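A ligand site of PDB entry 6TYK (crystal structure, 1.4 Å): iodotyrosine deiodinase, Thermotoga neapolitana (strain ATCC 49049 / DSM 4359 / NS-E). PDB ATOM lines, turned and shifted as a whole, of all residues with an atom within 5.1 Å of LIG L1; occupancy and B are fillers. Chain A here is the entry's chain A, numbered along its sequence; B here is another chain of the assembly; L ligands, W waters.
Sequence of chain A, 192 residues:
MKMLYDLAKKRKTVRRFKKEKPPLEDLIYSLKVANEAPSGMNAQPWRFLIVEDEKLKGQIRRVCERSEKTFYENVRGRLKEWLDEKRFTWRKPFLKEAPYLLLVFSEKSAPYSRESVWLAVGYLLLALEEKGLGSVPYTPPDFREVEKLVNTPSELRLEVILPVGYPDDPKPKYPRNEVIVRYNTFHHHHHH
The side-chain hydroxyl of Tyr 72 lies within hydrogen-bond range of an oxygen (O2) of LIG L1, 2.6 Å away. An oxygen (O2) of LIG L1 is in salt-bridge range of the side-chain amino group (NZ) of Lys 92, 2.6 Å away. The side-chain carboxylate (OE2) of Glu 68 is in salt-bridge range of a nitrogen (N1) of LIG L1. N of Met 41 of chain B is in hydrogen-bond range of O1 of LIG L1, 2.9 Å away. O of Thr 139 lies within hydrogen-bond range of N1 of LIG L1, 3.4 Å away. The backbone NH (N) of Thr 139 is in hydrogen-bond range of an oxygen (O2) of LG2 L2, 3.1 Å away. A nitrogen (N3) of LG2 L2 sits at hydrogen-bond distance from the side-chain hydroxyl of Thr 139, at 3.0 Å. The backbone NH (N) of Ser 39 of chain B sits at hydrogen-bond distance from an oxygen (O4) of LG2 L2 (3.3 Å). O4 of LG2 L2 sits close to O of Ser 39 of chain B (3.5 Å). NE of Arg 15 sits at hydrogen-bond distance from O1 of LG2 L2, 2.9 Å away.
Water W2 bridges OE1 of Glu 68 (2.9 Å) and N1 of LIG L1 (3.0 Å). Water W1 lies within hydrogen-bond range of an oxygen (O1) of LG2 L2 (2.7 Å), the side-chain amino group of Lys 92 (2.7 Å) and an oxygen (O3) of LIG L1 (3.4 Å).
CE2 of Phe 71 touches C2 of LIG L1, 3.9 Å away. Trp 82 touches LIG L1. Leu 83 touches LIG L1. Phe 88 touches LIG L1 (CE2 to C8, 3.8 Å). Thr 89 touches LIG L1 (O to O2, 3.9 Å). Tyr 138 touches LIG L1 (CE1 to O3, 3.3 Å). Gly 40 of chain B touches LIG L1 (CA to I1, 3.6 Å). Pro 111 of chain B touches LIG L1. Hydrophobic or aromatic side chains within 4 Å of LIG L1: Phe 71, Tyr 72, Trp 82, Leu 83, Phe 88, Tyr 138 and Pro 111 of chain B. 13 residues have an atom within 4 Å of LIG L1: Glu 68, Phe 71, Tyr 72, Trp 82, Leu 83, Phe 88, Thr 89, Lys 92, Tyr 138, Thr 139, Gly 40 of chain B, Met 41 of chain B and Pro 111 of chain B. The nearest printed residue that does not touch LIG L1 is Tyr 112 of chain B (4.1 Å).
The backbone carbonyl oxygen (O) of Thr 89 sits at hydrogen-bond distance from the side-chain amino group (NZ) of Lys 92. The side-chain hydroxyl (OH) of Tyr 138 sits at hydrogen-bond distance from the side-chain carboxylate (OE2) of Glu 68 (2.6 Å). O of Met 41 of chain B is in hydrogen-bond range of NE1 of Trp 82 (3.2 Å). O of Leu 83 lies within hydrogen-bond range of N of Phe 88 (2.9 Å).
An oxygen (O3) of LG2 L2 is in hydrogen-bond range of an oxygen (O1) of LIG L1, 2.6 Å away.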
ATOM      1  N   ARG A  15     -15.136  13.973  28.752  1.00  0.00           N
ATOM      2  CA  ARG A  15     -13.761  13.605  28.423  1.00  0.00           C
ATOM      3  C   ARG A  15     -12.830  14.773  28.706  1.00  0.00           C
ATOM      4  O   ARG A  15     -11.630  14.674  28.468  1.00  0.00           O
ATOM      5  CB  ARG A  15     -13.649  13.206  26.949  1.00  0.00           C
ATOM      6  CG  ARG A  15     -14.497  11.996  26.579  1.00  0.00           C
ATOM      7  CD  ARG A  15     -14.397  11.667  25.098  1.00  0.00           C
ATOM      8  NE  ARG A  15     -15.145  10.452  24.749  1.00  0.00           N
ATOM      9  CZ  ARG A  15     -16.388  10.438  24.283  1.00  0.00           C
ATOM     10  NH1 ARG A  15     -17.041  11.577  24.089  1.00  0.00           N
ATOM     11  NH2 ARG A  15     -16.961   9.284  23.996  1.00  0.00           N
ATOM     12  N   GLU A  68      -4.243   2.201  21.821  1.00  0.00           N
ATOM     13  CA  GLU A  68      -5.152   2.966  20.986  1.00  0.00           C
ATOM     14  C   GLU A  68      -4.500   3.340  19.656  1.00  0.00           C
ATOM     15  O   GLU A  68      -5.145   3.303  18.618  1.00  0.00           O
ATOM     16  CB  GLU A  68      -5.627   4.240  21.700  1.00  0.00           C
ATOM     17  CG  GLU A  68      -6.489   4.004  22.932  1.00  0.00           C
ATOM     18  CD  GLU A  68      -7.849   3.404  22.618  1.00  0.00           C
ATOM     19  OE1 GLU A  68      -8.086   3.001  21.460  1.00  0.00           O
ATOM     20  OE2 GLU A  68      -8.663   3.328  23.555  1.00  0.00           O
ATOM     21  N   PHE A  71      -4.677   0.495  17.462  1.00  0.00           N
ATOM     22  CA  PHE A  71      -6.085   0.319  17.130  1.00  0.00           C
ATOM     23  C   PHE A  71      -6.537   1.287  16.040  1.00  0.00           C
ATOM     24  O   PHE A  71      -7.157   0.889  15.058  1.00  0.00           O
ATOM     25  CB  PHE A  71      -6.934   0.491  18.395  1.00  0.00           C
ATOM     26  CG  PHE A  71      -8.405   0.652  18.135  1.00  0.00           C
ATOM     27  CD1 PHE A  71      -9.209  -0.446  17.889  1.00  0.00           C
ATOM     28  CD2 PHE A  71      -8.990   1.912  18.146  1.00  0.00           C
ATOM     29  CE1 PHE A  71     -10.569  -0.297  17.656  1.00  0.00           C
ATOM     30  CE2 PHE A  71     -10.337   2.066  17.915  1.00  0.00           C
ATOM     31  CZ  PHE A  71     -11.132   0.965  17.667  1.00  0.00           C
ATOM     32  N   TYR A  72      -6.195   2.566  16.200  1.00  0.00           N
ATOM     33  CA  TYR A  72      -6.589   3.571  15.204  1.00  0.00           C
ATOM     34  C   TYR A  72      -5.945   3.345  13.838  1.00  0.00           C
ATOM     35  O   TYR A  72      -6.517   3.711  12.815  1.00  0.00           O
ATOM     36  CB  TYR A  72      -6.317   4.987  15.728  1.00  0.00           C
ATOM     37  CG  TYR A  72      -7.457   5.514  16.574  1.00  0.00           C
ATOM     38  CD1 TYR A  72      -7.535   5.241  17.926  1.00  0.00           C
ATOM     39  CD2 TYR A  72      -8.479   6.230  15.985  1.00  0.00           C
ATOM     40  CE1 TYR A  72      -8.589   5.707  18.675  1.00  0.00           C
ATOM     41  CE2 TYR A  72      -9.534   6.701  16.725  1.00  0.00           C
ATOM     42  CZ  TYR A  72      -9.590   6.431  18.077  1.00  0.00           C
ATOM     43  OH  TYR A  72     -10.649   6.893  18.812  1.00  0.00           O
ATOM     44  N   LEU A  79     -17.185   1.129  13.359  1.00  0.00           N
ATOM     45  CA  LEU A  79     -16.563   1.865  14.453  1.00  0.00           C
ATOM     46  C   LEU A  79     -15.571   2.897  13.917  1.00  0.00           C
ATOM     47  O   LEU A  79     -15.512   4.026  14.411  1.00  0.00           O
ATOM     48  CB  LEU A  79     -15.886   0.907  15.446  1.00  0.00           C
ATOM     49  CG  LEU A  79     -15.276   1.534  16.700  1.00  0.00           C
ATOM     50  CD1 LEU A  79     -16.280   2.428  17.433  1.00  0.00           C
ATOM     51  CD2 LEU A  79     -14.725   0.454  17.640  1.00  0.00           C
ATOM     52  N   TRP A  82     -17.456   5.873  12.592  1.00  0.00           N
ATOM     53  CA  TRP A  82     -17.997   6.681  13.679  1.00  0.00           C
ATOM     54  C   TRP A  82     -16.898   7.503  14.351  1.00  0.00           C
ATOM     55  O   TRP A  82     -17.070   8.689  14.591  1.00  0.00           O
ATOM     56  CB  TRP A  82     -18.710   5.775  14.686  1.00  0.00           C
ATOM     57  CG  TRP A  82     -19.435   6.503  15.781  1.00  0.00           C
ATOM     58  CD1 TRP A  82     -20.713   6.977  15.737  1.00  0.00           C
ATOM     59  CD2 TRP A  82     -18.950   6.767  17.103  1.00  0.00           C
ATOM     60  NE1 TRP A  82     -21.045   7.555  16.941  1.00  0.00           N
ATOM     61  CE2 TRP A  82     -19.980   7.430  17.795  1.00  0.00           C
ATOM     62  CE3 TRP A  82     -17.745   6.527  17.757  1.00  0.00           C
ATOM     63  CZ2 TRP A  82     -19.845   7.859  19.114  1.00  0.00           C
ATOM     64  CZ3 TRP A  82     -17.604   6.944  19.069  1.00  0.00           C
ATOM     65  CH2 TRP A  82     -18.653   7.602  19.737  1.00  0.00           C
ATOM     66  N   LEU A  83     -15.766   6.855  14.658  1.00  0.00           N
ATOM     67  CA  LEU A  83     -14.652   7.550  15.285  1.00  0.00           C
ATOM     68  C   LEU A  83     -14.118   8.656  14.390  1.00  0.00           C
ATOM     69  O   LEU A  83     -13.788   9.742  14.857  1.00  0.00           O
ATOM     70  CB  LEU A  83     -13.525   6.582  15.615  1.00  0.00           C
ATOM     71  CG  LEU A  83     -13.881   5.534  16.672  1.00  0.00           C
ATOM     72  CD1 LEU A  83     -12.828   4.441  16.738  1.00  0.00           C
ATOM     73  CD2 LEU A  83     -14.088   6.159  18.060  1.00  0.00           C
ATOM     74  N   PHE A  88     -12.289  11.442  16.721  1.00  0.00           N
ATOM     75  CA  PHE A  88     -11.585  10.801  17.824  1.00  0.00           C
ATOM     76  C   PHE A  88     -10.133  10.525  17.434  1.00  0.00           C
ATOM     77  O   PHE A  88      -9.838  10.295  16.260  1.00  0.00           O
ATOM     78  CB  PHE A  88     -12.252   9.472  18.170  1.00  0.00           C
ATOM     79  CG  PHE A  88     -13.461   9.587  19.064  1.00  0.00           C
ATOM     80  CD1 PHE A  88     -14.632  10.159  18.607  1.00  0.00           C
ATOM     81  CD2 PHE A  88     -13.429   9.065  20.341  1.00  0.00           C
ATOM     82  CE1 PHE A  88     -15.740  10.242  19.429  1.00  0.00           C
ATOM     83  CE2 PHE A  88     -14.528   9.150  21.152  1.00  0.00           C
ATOM     84  CZ  PHE A  88     -15.684   9.736  20.701  1.00  0.00           C
ATOM     85  N   THR A  89      -9.249  10.514  18.412  1.00  0.00           N
ATOM     86  CA  THR A  89      -7.857  10.133  18.165  1.00  0.00           C
ATOM     87  C   THR A  89      -7.354   9.230  19.296  1.00  0.00           C
ATOM     88  O   THR A  89      -8.036   9.057  20.316  1.00  0.00           O
ATOM     89  CB  THR A  89      -6.935  11.365  18.084  1.00  0.00           C
ATOM     90  OG1 THR A  89      -6.915  12.022  19.354  1.00  0.00           O
ATOM     91  CG2 THR A  89      -7.425  12.322  17.027  1.00  0.00           C
ATOM     92  N   LYS A  92      -5.158  10.219  24.819  1.00  0.00           N
ATOM     93  CA  LYS A  92      -6.156  10.131  25.892  1.00  0.00           C
ATOM     94  C   LYS A  92      -5.783  11.045  27.060  1.00  0.00           C
ATOM     95  O   LYS A  92      -5.452  10.569  28.150  1.00  0.00           O
ATOM     96  CB  LYS A  92      -6.309   8.686  26.365  1.00  0.00           C
ATOM     97  CG  LYS A  92      -6.822   7.728  25.290  1.00  0.00           C
ATOM     98  CD  LYS A  92      -8.150   8.184  24.695  1.00  0.00           C
ATOM     99  CE  LYS A  92      -8.399   7.591  23.300  1.00  0.00           C
ATOM    100  NZ  LYS A  92      -9.531   8.257  22.593  1.00  0.00           N
ATOM    101  N   TYR A 138     -14.291   4.201  29.751  1.00  0.00           N
ATOM    102  CA  TYR A 138     -13.195   4.049  28.836  1.00  0.00           C
ATOM    103  C   TYR A 138     -12.769   2.591  28.734  1.00  0.00           C
ATOM    104  O   TYR A 138     -12.508   1.944  29.752  1.00  0.00           O
ATOM    105  CB  TYR A 138     -12.033   4.952  29.239  1.00  0.00           C
ATOM    106  CG  TYR A 138     -10.843   4.736  28.349  1.00  0.00           C
ATOM    107  CD1 TYR A 138     -10.953   4.929  26.984  1.00  0.00           C
ATOM    108  CD2 TYR A 138      -9.630   4.284  28.867  1.00  0.00           C
ATOM    109  CE1 TYR A 138      -9.891   4.701  26.157  1.00  0.00           C
ATOM    110  CE2 TYR A 138      -8.558   4.053  28.037  1.00  0.00           C
ATOM    111  CZ  TYR A 138      -8.693   4.263  26.683  1.00  0.00           C
ATOM    112  OH  TYR A 138      -7.635   4.031  25.843  1.00  0.00           O
ATOM    113  N   THR A 139     -12.765   2.078  27.516  1.00  0.00           N
ATOM    114  CA  THR A 139     -12.453   0.678  27.275  1.00  0.00           C
ATOM    115  C   THR A 139     -11.340   0.574  26.247  1.00  0.00           C
ATOM    116  O   THR A 139     -11.595   0.548  25.041  1.00  0.00           O
ATOM    117  CB  THR A 139     -13.703  -0.090  26.793  1.00  0.00           C
ATOM    118  OG1 THR A 139     -14.228   0.553  25.628  1.00  0.00           O
ATOM    119  CG2 THR A 139     -14.773  -0.100  27.869  1.00  0.00           C
ATOM    120  N   PRO A 140     -10.081   0.532  26.717  1.00  0.00           N
ATOM    121  CA  PRO A 140      -8.934   0.440  25.806  1.00  0.00           C
ATOM    122  C   PRO A 140      -8.922  -0.916  25.105  1.00  0.00           C
ATOM    123  O   PRO A 140      -9.591  -1.840  25.553  1.00  0.00           O
ATOM    124  CB  PRO A 140      -7.730   0.561  26.744  1.00  0.00           C
ATOM    125  CG  PRO A 140      -8.228   0.033  28.058  1.00  0.00           C
ATOM    126  CD  PRO A 140      -9.678   0.473  28.137  1.00  0.00           C
ATOM    127  N   SER B  39     -23.663   4.199  25.494  1.00  0.00           N
ATOM    128  CA  SER B  39     -23.463   2.906  24.865  1.00  0.00           C
ATOM    129  C   SER B  39     -22.244   3.003  23.968  1.00  0.00           C
ATOM    130  O   SER B  39     -21.889   4.095  23.526  1.00  0.00           O
ATOM    131  CB  SER B  39     -24.703   2.463  24.078  1.00  0.00           C
ATOM    132  OG  SER B  39     -25.001   3.368  23.031  1.00  0.00           O
ATOM    133  N   GLY B  40     -21.589   1.874  23.701  1.00  0.00           N
ATOM    134  CA  GLY B  40     -20.444   1.876  22.796  1.00  0.00           C
ATOM    135  C   GLY B  40     -20.838   2.499  21.460  1.00  0.00           C
ATOM    136  O   GLY B  40     -21.872   2.160  20.890  1.00  0.00           O
ATOM    137  N   MET B  41     -19.993   3.422  20.983  1.00  0.00           N
ATOM    138  CA  MET B  41     -20.230   4.235  19.778  1.00  0.00           C
ATOM    139  C   MET B  41     -21.648   4.794  19.634  1.00  0.00           C
ATOM    140  O   MET B  41     -22.127   5.005  18.530  1.00  0.00           O
ATOM    141  CB  MET B  41     -19.743   3.558  18.495  1.00  0.00           C
ATOM    142  CG  MET B  41     -20.471   2.301  18.020  1.00  0.00           C
ATOM    143  SD  MET B  41     -20.048   1.916  16.273  1.00  0.00           S
ATOM    144  CE  MET B  41     -21.024   3.176  15.435  1.00  0.00           C
ATOM    145  N   ASN B  42     -22.270   5.073  20.775  1.00  0.00           N
ATOM    146  CA  ASN B  42     -23.646   5.555  20.801  1.00  0.00           C
ATOM    147  C   ASN B  42     -24.587   4.718  19.923  1.00  0.00           C
ATOM    148  O   ASN B  42     -25.534   5.235  19.358  1.00  0.00           O
ATOM    149  CB  ASN B  42     -23.728   7.029  20.424  1.00  0.00           C
ATOM    150  CG  ASN B  42     -25.061   7.647  20.791  1.00  0.00           C
ATOM    151  OD1 ASN B  42     -25.669   7.274  21.789  1.00  0.00           O
ATOM    152  ND2 ASN B  42     -25.529   8.566  19.984  1.00  0.00           N
ATOM    153  N   PRO B 111     -20.362  -2.479  18.954  1.00  0.00           N
ATOM    154  CA  PRO B 111     -19.231  -2.542  19.868  1.00  0.00           C
ATOM    155  C   PRO B 111     -19.692  -2.461  21.321  1.00  0.00           C
ATOM    156  O   PRO B 111     -20.444  -1.549  21.675  1.00  0.00           O
ATOM    157  CB  PRO B 111     -18.430  -1.271  19.524  1.00  0.00           C
ATOM    158  CG  PRO B 111     -18.865  -0.899  18.150  1.00  0.00           C
ATOM    159  CD  PRO B 111     -20.295  -1.314  18.056  1.00  0.00           C
ATOM    160  N   TYR B 112     -19.240  -3.389  22.159  1.00  0.00           N
ATOM    161  CA  TYR B 112     -19.608  -3.388  23.571  1.00  0.00           C
ATOM    162  C   TYR B 112     -21.124  -3.402  23.756  1.00  0.00           C
ATOM    163  O   TYR B 112     -21.667  -2.797  24.699  1.00  0.00           O
ATOM    164  CB  TYR B 112     -18.975  -2.203  24.300  1.00  0.00           C
ATOM    165  CG  TYR B 112     -17.544  -2.490  24.680  1.00  0.00           C
ATOM    166  CD1 TYR B 112     -16.518  -2.337  23.764  1.00  0.00           C
ATOM    167  CD2 TYR B 112     -17.227  -2.952  25.950  1.00  0.00           C
ATOM    168  CE1 TYR B 112     -15.204  -2.627  24.108  1.00  0.00           C
ATOM    169  CE2 TYR B 112     -15.922  -3.244  26.305  1.00  0.00           C
ATOM    170  CZ  TYR B 112     -14.916  -3.076  25.376  1.00  0.00           C
ATOM    171  OH  TYR B 112     -13.604  -3.357  25.702  1.00  0.00           O
HETATM  172  N1  LIG L   1     -11.419   3.158  22.832  1.00  0.00           N
HETATM  173  C1  LIG L   1     -11.248   4.001  21.673  1.00  0.00           C
HETATM  174  C2  LIG L   1     -12.359   3.937  20.609  1.00  0.00           C
HETATM  175  C3  LIG L   1     -13.749   4.109  21.109  1.00  0.00           C
HETATM  176  C4  LIG L   1     -14.554   2.981  21.313  1.00  0.00           C
HETATM  177  C5  LIG L   1     -15.878   3.075  21.742  1.00  0.00           C
HETATM  178  I1  LIG L   1     -16.925   1.382  22.044  1.00  0.00           I
HETATM  179  C6  LIG L   1     -16.416   4.341  21.968  1.00  0.00           C
HETATM  180  O1  LIG L   1     -17.703   4.531  22.387  1.00  0.00           O
HETATM  181  C7  LIG L   1     -15.632   5.494  21.779  1.00  0.00           C
HETATM  182  C8  LIG L   1     -14.319   5.375  21.338  1.00  0.00           C
HETATM  183  C9  LIG L   1     -11.089   5.461  22.038  1.00  0.00           C
HETATM  184  O2  LIG L   1     -10.777   6.399  21.314  1.00  0.00           O
HETATM  185  O3  LIG L   1     -11.313   5.734  23.354  1.00  0.00           O
HETATM  186  N1  LG2 L   2     -15.871   6.530  24.981  1.00  0.00           N
HETATM  187  C1  LG2 L   2     -14.568   6.696  24.625  1.00  0.00           C
HETATM  188  O1  LG2 L   2     -14.151   7.806  24.358  1.00  0.00           O
HETATM  189  N2  LG2 L   2     -13.710   5.620  24.583  1.00  0.00           N
HETATM  190  C2  LG2 L   2     -14.157   4.360  24.864  1.00  0.00           C
HETATM  191  O2  LG2 L   2     -13.369   3.412  24.818  1.00  0.00           O
HETATM  192  C3  LG2 L   2     -15.490   4.185  25.241  1.00  0.00           C
HETATM  193  N3  LG2 L   2     -15.970   2.936  25.554  1.00  0.00           N
HETATM  194  C4  LG2 L   2     -17.291   2.781  25.953  1.00  0.00           C
HETATM  195  C5  LG2 L   2     -17.750   1.512  26.287  1.00  0.00           C
HETATM  196  C6  LG2 L   2     -19.061   1.313  26.695  1.00  0.00           C
HETATM  197  C7  LG2 L   2     -19.508  -0.080  27.053  1.00  0.00           C
HETATM  198  C8  LG2 L   2     -19.920   2.403  26.756  1.00  0.00           C
HETATM  199  C9  LG2 L   2     -21.349   2.216  27.193  1.00  0.00           C
HETATM  200  C10 LG2 L   2     -19.462   3.673  26.422  1.00  0.00           C
HETATM  201  C11 LG2 L   2     -18.142   3.869  26.012  1.00  0.00           C
HETATM  202  N4  LG2 L   2     -17.670   5.134  25.651  1.00  0.00           N
HETATM  203  C12 LG2 L   2     -16.343   5.293  25.311  1.00  0.00           C
HETATM  204  C13 LG2 L   2     -18.563   6.341  25.698  1.00  0.00           C
HETATM  205  C14 LG2 L   2     -19.499   6.357  24.467  1.00  0.00           C
HETATM  206  O3  LG2 L   2     -18.809   6.757  23.294  1.00  0.00           O
HETATM  207  C15 LG2 L   2     -20.690   7.262  24.757  1.00  0.00           C
HETATM  208  O4  LG2 L   2     -21.437   6.675  25.802  1.00  0.00           O
HETATM  209  C16 LG2 L   2     -21.599   7.494  23.547  1.00  0.00           C
HETATM  210  O5  LG2 L   2     -20.885   8.218  22.545  1.00  0.00           O
HETATM  211  C17 LG2 L   2     -22.839   8.286  23.942  1.00  0.00           C
HETATM  212  O6  LG2 L   2     -22.446   9.478  24.573  1.00  0.00           O
HETATM  213  P1  LG2 L   2     -23.528  10.548  25.089  1.00  0.00           P
HETATM  214  O7  LG2 L   2     -22.691  11.732  25.571  1.00  0.00           O
HETATM  215  O8  LG2 L   2     -24.266   9.957  26.256  1.00  0.00           O
HETATM  216  O9  LG2 L   2     -24.408  10.917  23.915  1.00  0.00           O
HETATM  217  O   HOH W   1     -11.893   9.105  23.705  1.00  0.00           O
HETATM  218  O   HOH W   2     -10.177   1.074  21.033  1.00  0.00           O
